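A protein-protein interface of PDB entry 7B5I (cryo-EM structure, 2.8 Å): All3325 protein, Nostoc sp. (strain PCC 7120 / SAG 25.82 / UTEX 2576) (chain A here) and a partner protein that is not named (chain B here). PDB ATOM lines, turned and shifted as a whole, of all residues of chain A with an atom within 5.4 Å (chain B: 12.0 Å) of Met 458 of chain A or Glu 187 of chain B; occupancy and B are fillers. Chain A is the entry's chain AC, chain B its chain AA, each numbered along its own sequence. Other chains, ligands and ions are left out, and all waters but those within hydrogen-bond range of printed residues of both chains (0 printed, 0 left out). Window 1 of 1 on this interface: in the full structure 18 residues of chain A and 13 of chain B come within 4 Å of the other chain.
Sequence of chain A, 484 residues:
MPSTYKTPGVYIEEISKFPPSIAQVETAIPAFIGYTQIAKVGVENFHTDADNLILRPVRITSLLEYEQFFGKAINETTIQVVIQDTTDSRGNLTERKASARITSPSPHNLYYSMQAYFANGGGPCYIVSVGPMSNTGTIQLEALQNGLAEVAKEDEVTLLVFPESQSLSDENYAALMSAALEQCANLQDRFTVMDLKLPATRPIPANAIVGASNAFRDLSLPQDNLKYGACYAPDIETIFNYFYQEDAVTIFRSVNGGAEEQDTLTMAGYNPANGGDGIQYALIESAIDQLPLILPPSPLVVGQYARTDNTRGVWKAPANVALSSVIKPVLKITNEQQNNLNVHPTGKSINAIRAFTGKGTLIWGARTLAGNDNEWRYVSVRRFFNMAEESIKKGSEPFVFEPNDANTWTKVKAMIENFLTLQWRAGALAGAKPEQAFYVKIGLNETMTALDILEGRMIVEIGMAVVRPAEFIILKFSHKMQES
The backbone carbonyl oxygen of Ser 183 of chain B sits at hydrogen-bond distance from the backbone NH of Asn 404 of chain A (3.3 Å). The backbone carbonyl oxygen (O) of Gly 456 of chain A is in hydrogen-bond range of the backbone NH (N) of Thr 186 of chain B (3.0 Å). The backbone NH (N) of Glu 187 of chain B lies within hydrogen-bond range of the backbone carbonyl oxygen (O) of Gly 456 of chain A. N of Met 458 of chain A is in hydrogen-bond range of O of Glu 187 of chain B (3.0 Å). The backbone NH of Tyr 189 of chain B is in hydrogen-bond range of the backbone carbonyl oxygen of Met 458 of chain A (3.0 Å). The backbone carbonyl oxygen (O) of Tyr 189 of chain B lies within hydrogen-bond range of the backbone NH (N) of Val 460 of chain A (3.4 Å). O of Val 460 of chain A lies within hydrogen-bond range of N of Asn 191 of chain B (3.3 Å).
The side-chain hydroxyl (OG1) of Thr 184 of chain B is in hydrogen-bond range of the backbone carbonyl oxygen (O) of Gly 76 of chain B, 3.2 Å away. The side-chain amide oxygen (OD1) of Asn 404 of chain A sits at hydrogen-bond distance from the indole nitrogen (NE1) of Trp 409 of chain A (3.0 Å). The side-chain amide nitrogen of Asn 404 of chain A sits at hydrogen-bond distance from the backbone carbonyl oxygen of Arg 457 of chain A (3.4 Å).
Ile 185 of chain B touches Asn 404 of chain A (CG1 to CB, 3.98 Å). CG2 of Thr 408 of chain A touches CD1 of Ile 185 of chain B (3.9 Å). O of Thr 184 of chain B touches CA of Gly 456 of chain A, at 3.5 Å. Gly 456 of chain A touches Ile 185 of chain B (O to CA, 3.8 Å). O of Glu 187 of chain B touches CA of Arg 457 of chain A, 3.4 Å away. CD of Arg 457 of chain A touches CE2 of Tyr 189 of chain B, at 3.4 Å. Ile 185 of chain B touches Met 458 of chain A (CD1 to SD, 3.98 Å). CA of Ile 188 of chain B touches O of Met 458 of chain A, 3.4 Å away. Ile 459 of chain A touches Tyr 189 of chain B.
Printed residues of chain B within 4 Å of Met 458 of chain A: Ile 185, Glu 187, Ile 188 and Tyr 189. Glu 187 of chain B touches three residues of chain A. Of chain B, only Ser 183 (3.3 Å) and Ile 185 (3.98 Å) come within 4 Å of Asn 404 of chain A. Of chain B, only Ile 185 comes within 4 Å of Thr 408 of chain A. Of chain B, only Thr 184, Ile 185, Thr 186 and Glu 187 come within 4 Å of Gly 456 of chain A. Arg 457 of chain A touches just these residues of chain B: Glu 187 and Tyr 189. Ile 459 of chain A touches just one residue of chain B: Tyr 189 (3.6 Å). Val 460 of chain A touches just these residues of chain B: Tyr 189 and Asn 191. Of the printed residues of chain A, Asn 191 of chain B touches Val 460 (3.3 Å). Of the printed residues of chain A, Ser 183 of chain B touches Asn 404. Of the printed residues of chain A, Thr 184 of chain B touches Gly 456. Of the printed residues of chain A, Tyr 189 of chain B touches Arg 457, Met 458, Ile 459 and Val 460. Met 448 of chain A touches none of the printed residues of chain B. Val 412 of chain A touches none of the printed residues of chain B. The nearest printed residue of chain A that does not touch Tyr 189 of chain B is Ile 442 of chain A (7.7 Å).
Of the 10 printed residues of chain B, 8 touch a printed residue of chain A. Hydrophobic or aromatic side chains of chain B within 4 Å of the printed part of chain A: Ile 185, Ile 188 and Tyr 189. Of the 11 printed residues of chain A, 7 touch a printed residue of chain B. Printed residues of chain A that touch a printed residue of chain B: Asn 404, Thr 408, Gly 456, Arg 457, Met 458, Ile 459 and Val 460. Among the printed residues, no Asp or Glu carboxylate lies within 4 Å of a Lys or Arg side-chain nitrogen of the other chain.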
ATOM      1  N   ASN A 404      10.270 -31.702  13.048  1.00  0.00           N
ATOM      2  CA  ASN A 404       9.980 -31.255  11.686  1.00  0.00           C
ATOM      3  C   ASN A 404      11.034 -31.832  10.744  1.00  0.00           C
ATOM      4  O   ASN A 404      11.968 -31.156  10.303  1.00  0.00           O
ATOM      5  CB  ASN A 404       9.941 -29.732  11.636  1.00  0.00           C
ATOM      6  CG  ASN A 404       9.243 -29.206  10.403  1.00  0.00           C
ATOM      7  OD1 ASN A 404       8.723 -29.969   9.595  1.00  0.00           O
ATOM      8  ND2 ASN A 404       9.227 -27.892  10.254  1.00  0.00           N
ATOM      9  N   THR A 408       8.151 -37.527   9.836  1.00  0.00           N
ATOM     10  CA  THR A 408       6.814 -36.989  10.032  1.00  0.00           C
ATOM     11  C   THR A 408       6.158 -36.673   8.696  1.00  0.00           C
ATOM     12  O   THR A 408       4.957 -36.908   8.512  1.00  0.00           O
ATOM     13  CB  THR A 408       6.892 -35.740  10.903  1.00  0.00           C
ATOM     14  OG1 THR A 408       7.532 -36.066  12.139  1.00  0.00           O
ATOM     15  CG2 THR A 408       5.512 -35.223  11.194  1.00  0.00           C
ATOM     16  N   TRP A 409       6.930 -36.133   7.756  1.00  0.00           N
ATOM     17  CA  TRP A 409       6.389 -35.805   6.445  1.00  0.00           C
ATOM     18  C   TRP A 409       5.893 -37.054   5.733  1.00  0.00           C
ATOM     19  O   TRP A 409       4.813 -37.051   5.124  1.00  0.00           O
ATOM     20  CB  TRP A 409       7.462 -35.101   5.618  1.00  0.00           C
ATOM     21  CG  TRP A 409       7.998 -33.869   6.266  1.00  0.00           C
ATOM     22  CD1 TRP A 409       7.411 -33.141   7.256  1.00  0.00           C
ATOM     23  CD2 TRP A 409       9.242 -33.221   5.977  1.00  0.00           C
ATOM     24  NE1 TRP A 409       8.207 -32.079   7.596  1.00  0.00           N
ATOM     25  CE2 TRP A 409       9.339 -32.107   6.827  1.00  0.00           C
ATOM     26  CE3 TRP A 409      10.282 -33.476   5.081  1.00  0.00           C
ATOM     27  CZ2 TRP A 409      10.434 -31.252   6.806  1.00  0.00           C
ATOM     28  CZ3 TRP A 409      11.368 -32.627   5.068  1.00  0.00           C
ATOM     29  CH2 TRP A 409      11.436 -31.532   5.922  1.00  0.00           C
ATOM     30  N   VAL A 412       2.548 -38.146   7.391  1.00  0.00           N
ATOM     31  CA  VAL A 412       1.446 -37.261   7.034  1.00  0.00           C
ATOM     32  C   VAL A 412       0.987 -37.526   5.608  1.00  0.00           C
ATOM     33  O   VAL A 412      -0.221 -37.613   5.326  1.00  0.00           O
ATOM     34  CB  VAL A 412       1.879 -35.798   7.226  1.00  0.00           C
ATOM     35  CG1 VAL A 412       0.827 -34.854   6.693  1.00  0.00           C
ATOM     36  CG2 VAL A 412       2.152 -35.518   8.683  1.00  0.00           C
ATOM     37  N   ILE A 442       4.642 -32.441  -0.155  1.00  0.00           N
ATOM     38  CA  ILE A 442       5.183 -31.967   1.118  1.00  0.00           C
ATOM     39  C   ILE A 442       6.676 -32.270   1.236  1.00  0.00           C
ATOM     40  O   ILE A 442       7.081 -33.436   1.240  1.00  0.00           O
ATOM     41  CB  ILE A 442       4.402 -32.563   2.307  1.00  0.00           C
ATOM     42  CG1 ILE A 442       5.059 -32.139   3.619  1.00  0.00           C
ATOM     43  CG2 ILE A 442       4.264 -34.073   2.198  1.00  0.00           C
ATOM     44  CD1 ILE A 442       4.253 -32.459   4.840  1.00  0.00           C
ATOM     45  N   MET A 448       8.761 -26.274   0.824  1.00  0.00           N
ATOM     46  CA  MET A 448       9.340 -25.816   2.078  1.00  0.00           C
ATOM     47  C   MET A 448      10.789 -25.412   1.867  1.00  0.00           C
ATOM     48  O   MET A 448      11.410 -25.779   0.870  1.00  0.00           O
ATOM     49  CB  MET A 448       9.240 -26.900   3.162  1.00  0.00           C
ATOM     50  CG  MET A 448       7.826 -27.136   3.673  1.00  0.00           C
ATOM     51  SD  MET A 448       7.693 -28.553   4.765  1.00  0.00           S
ATOM     52  CE  MET A 448       8.603 -27.956   6.170  1.00  0.00           C
ATOM     53  N   GLY A 456       9.371 -23.544  12.166  1.00  0.00           N
ATOM     54  CA  GLY A 456       8.455 -24.549  12.659  1.00  0.00           C
ATOM     55  C   GLY A 456       7.195 -24.728  11.840  1.00  0.00           C
ATOM     56  O   GLY A 456       6.197 -25.212  12.380  1.00  0.00           O
ATOM     57  N   ARG A 457       7.212 -24.359  10.563  1.00  0.00           N
ATOM     58  CA  ARG A 457       6.046 -24.421   9.695  1.00  0.00           C
ATOM     59  C   ARG A 457       6.116 -25.631   8.774  1.00  0.00           C
ATOM     60  O   ARG A 457       7.187 -25.990   8.281  1.00  0.00           O
ATOM     61  CB  ARG A 457       5.926 -23.148   8.855  1.00  0.00           C
ATOM     62  CG  ARG A 457       5.541 -21.922   9.654  1.00  0.00           C
ATOM     63  CD  ARG A 457       5.116 -20.768   8.763  1.00  0.00           C
ATOM     64  NE  ARG A 457       6.217 -20.227   7.984  1.00  0.00           N
ATOM     65  CZ  ARG A 457       7.031 -19.279   8.428  1.00  0.00           C
ATOM     66  NH1 ARG A 457       6.854 -18.775   9.638  1.00  0.00           N
ATOM     67  NH2 ARG A 457       8.018 -18.836   7.665  1.00  0.00           N
ATOM     68  N   MET A 458       4.965 -26.259   8.553  1.00  0.00           N
ATOM     69  CA  MET A 458       4.817 -27.351   7.602  1.00  0.00           C
ATOM     70  C   MET A 458       3.802 -26.940   6.549  1.00  0.00           C
ATOM     71  O   MET A 458       2.713 -26.472   6.888  1.00  0.00           O
ATOM     72  CB  MET A 458       4.365 -28.633   8.297  1.00  0.00           C
ATOM     73  CG  MET A 458       4.946 -29.891   7.695  1.00  0.00           C
ATOM     74  SD  MET A 458       4.531 -31.384   8.608  1.00  0.00           S
ATOM     75  CE  MET A 458       2.849 -31.024   9.092  1.00  0.00           C
ATOM     76  N   ILE A 459       4.183 -27.078   5.283  1.00  0.00           N
ATOM     77  CA  ILE A 459       3.318 -26.711   4.171  1.00  0.00           C
ATOM     78  C   ILE A 459       3.029 -27.921   3.294  1.00  0.00           C
ATOM     79  O   ILE A 459       3.943 -28.613   2.845  1.00  0.00           O
ATOM     80  CB  ILE A 459       3.946 -25.600   3.310  1.00  0.00           C
ATOM     81  CG1 ILE A 459       4.303 -24.391   4.177  1.00  0.00           C
ATOM     82  CG2 ILE A 459       3.001 -25.198   2.188  1.00  0.00           C
ATOM     83  CD1 ILE A 459       4.920 -23.246   3.404  1.00  0.00           C
ATOM     84  N   VAL A 460       1.747 -28.168   3.057  1.00  0.00           N
ATOM     85  CA  VAL A 460       1.312 -29.299   2.239  1.00  0.00           C
ATOM     86  C   VAL A 460       0.398 -28.780   1.133  1.00  0.00           C
ATOM     87  O   VAL A 460      -0.460 -27.927   1.382  1.00  0.00           O
ATOM     88  CB  VAL A 460       0.615 -30.383   3.090  1.00  0.00           C
ATOM     89  CG1 VAL A 460      -0.654 -29.845   3.728  1.00  0.00           C
ATOM     90  CG2 VAL A 460       0.310 -31.619   2.268  1.00  0.00           C
ATOM     91  N   GLY B  76      10.784 -28.179  23.722  1.00  0.00           N
ATOM     92  CA  GLY B  76      10.303 -27.905  22.385  1.00  0.00           C
ATOM     93  C   GLY B  76      11.342 -28.007  21.295  1.00  0.00           C
ATOM     94  O   GLY B  76      11.106 -27.511  20.189  1.00  0.00           O
ATOM     95  N   SER B 183      14.206 -28.406  15.522  1.00  0.00           N
ATOM     96  CA  SER B 183      13.016 -27.781  16.084  1.00  0.00           C
ATOM     97  C   SER B 183      11.768 -28.567  15.698  1.00  0.00           C
ATOM     98  O   SER B 183      11.776 -29.364  14.759  1.00  0.00           O
ATOM     99  CB  SER B 183      12.874 -26.321  15.627  1.00  0.00           C
ATOM    100  OG  SER B 183      12.616 -26.235  14.239  1.00  0.00           O
ATOM    101  N   THR B 184      10.686 -28.328  16.440  1.00  0.00           N
ATOM    102  CA  THR B 184       9.446 -29.079  16.308  1.00  0.00           C
ATOM    103  C   THR B 184       8.408 -28.302  15.502  1.00  0.00           C
ATOM    104  O   THR B 184       8.658 -27.207  14.996  1.00  0.00           O
ATOM    105  CB  THR B 184       8.887 -29.445  17.684  1.00  0.00           C
ATOM    106  OG1 THR B 184       8.558 -28.251  18.401  1.00  0.00           O
ATOM    107  CG2 THR B 184       9.900 -30.247  18.483  1.00  0.00           C
ATOM    108  N   ILE B 185       7.219 -28.891  15.388  1.00  0.00           N
ATOM    109  CA  ILE B 185       6.141 -28.362  14.558  1.00  0.00           C
ATOM    110  C   ILE B 185       5.229 -27.481  15.398  1.00  0.00           C
ATOM    111  O   ILE B 185       4.758 -27.896  16.460  1.00  0.00           O
ATOM    112  CB  ILE B 185       5.343 -29.506  13.914  1.00  0.00           C
ATOM    113  CG1 ILE B 185       6.195 -30.226  12.873  1.00  0.00           C
ATOM    114  CG2 ILE B 185       4.069 -28.989  13.292  1.00  0.00           C
ATOM    115  CD1 ILE B 185       5.618 -31.548  12.436  1.00  0.00           C
ATOM    116  N   THR B 186       4.954 -26.271  14.911  1.00  0.00           N
ATOM    117  CA  THR B 186       4.073 -25.346  15.614  1.00  0.00           C
ATOM    118  C   THR B 186       3.024 -24.682  14.726  1.00  0.00           C
ATOM    119  O   THR B 186       2.044 -24.152  15.259  1.00  0.00           O
ATOM    120  CB  THR B 186       4.899 -24.254  16.313  1.00  0.00           C
ATOM    121  OG1 THR B 186       6.030 -24.855  16.951  1.00  0.00           O
ATOM    122  CG2 THR B 186       4.075 -23.562  17.386  1.00  0.00           C
ATOM    123  N   GLU B 187       3.174 -24.710  13.406  1.00  0.00           N
ATOM    124  CA  GLU B 187       2.195 -24.103  12.515  1.00  0.00           C
ATOM    125  C   GLU B 187       2.068 -24.955  11.264  1.00  0.00           C
ATOM    126  O   GLU B 187       3.056 -25.524  10.796  1.00  0.00           O
ATOM    127  CB  GLU B 187       2.587 -22.673  12.136  1.00  0.00           C
ATOM    128  CG  GLU B 187       1.543 -21.952  11.307  1.00  0.00           C
ATOM    129  CD  GLU B 187       1.925 -20.523  10.998  1.00  0.00           C
ATOM    130  OE1 GLU B 187       3.048 -20.113  11.357  1.00  0.00           O
ATOM    131  OE2 GLU B 187       1.092 -19.802  10.411  1.00  0.00           O
ATOM    132  N   ILE B 188       0.857 -25.059  10.698  1.00  0.00           N
ATOM    133  CA  ILE B 188       0.591 -25.846   9.472  1.00  0.00           C
ATOM    134  C   ILE B 188      -0.294 -25.078   8.455  1.00  0.00           C
ATOM    135  O   ILE B 188      -1.271 -24.444   8.855  1.00  0.00           O
ATOM    136  CB  ILE B 188      -0.101 -27.197   9.814  1.00  0.00           C
ATOM    137  CG1 ILE B 188       0.745 -28.039  10.773  1.00  0.00           C
ATOM    138  CG2 ILE B 188      -0.387 -28.018   8.564  1.00  0.00           C
ATOM    139  CD1 ILE B 188       0.119 -29.368  11.133  1.00  0.00           C
ATOM    140  N   TYR B 189       0.060 -25.085   7.170  1.00  0.00           N
ATOM    141  CA  TYR B 189      -0.768 -24.456   6.152  1.00  0.00           C
ATOM    142  C   TYR B 189      -1.264 -25.563   5.294  1.00  0.00           C
ATOM    143  O   TYR B 189      -0.498 -26.414   4.923  1.00  0.00           O
ATOM    144  CB  TYR B 189      -0.016 -23.569   5.169  1.00  0.00           C
ATOM    145  CG  TYR B 189       0.670 -22.303   5.650  1.00  0.00           C
ATOM    146  CD1 TYR B 189       0.010 -21.104   5.738  1.00  0.00           C
ATOM    147  CD2 TYR B 189       2.004 -22.334   5.972  1.00  0.00           C
ATOM    148  CE1 TYR B 189       0.649 -19.984   6.170  1.00  0.00           C
ATOM    149  CE2 TYR B 189       2.658 -21.224   6.411  1.00  0.00           C
ATOM    150  CZ  TYR B 189       1.975 -20.046   6.508  1.00  0.00           C
ATOM    151  OH  TYR B 189       2.639 -18.936   6.943  1.00  0.00           O
ATOM    152  N   ILE B 190      -2.547 -25.521   4.961  1.00  0.00           N
ATOM    153  CA  ILE B 190      -3.152 -26.501   4.076  1.00  0.00           C
ATOM    154  C   ILE B 190      -3.627 -25.658   2.903  1.00  0.00           C
ATOM    155  O   ILE B 190      -4.485 -24.791   3.095  1.00  0.00           O
ATOM    156  CB  ILE B 190      -4.348 -27.207   4.729  1.00  0.00           C
ATOM    157  CG1 ILE B 190      -3.901 -27.963   5.983  1.00  0.00           C
ATOM    158  CG2 ILE B 190      -5.011 -28.156   3.742  1.00  0.00           C
ATOM    159  CD1 ILE B 190      -5.019 -28.708   6.678  1.00  0.00           C
ATOM    160  N   ASN B 191      -3.058 -25.890   1.715  1.00  0.00           N
ATOM    161  CA  ASN B 191      -3.399 -25.119   0.519  1.00  0.00           C
ATOM    162  C   ASN B 191      -3.320 -23.622   0.790  1.00  0.00           C
ATOM    163  O   ASN B 191      -4.135 -22.837   0.303  1.00  0.00           O
ATOM    164  CB  ASN B 191      -4.777 -25.504  -0.018  1.00  0.00           C
ATOM    165  CG  ASN B 191      -4.826 -26.924  -0.524  1.00  0.00           C
ATOM    166  OD1 ASN B 191      -3.819 -27.629  -0.521  1.00  0.00           O
ATOM    167  ND2 ASN B 191      -5.999 -27.354  -0.964  1.00  0.00           N
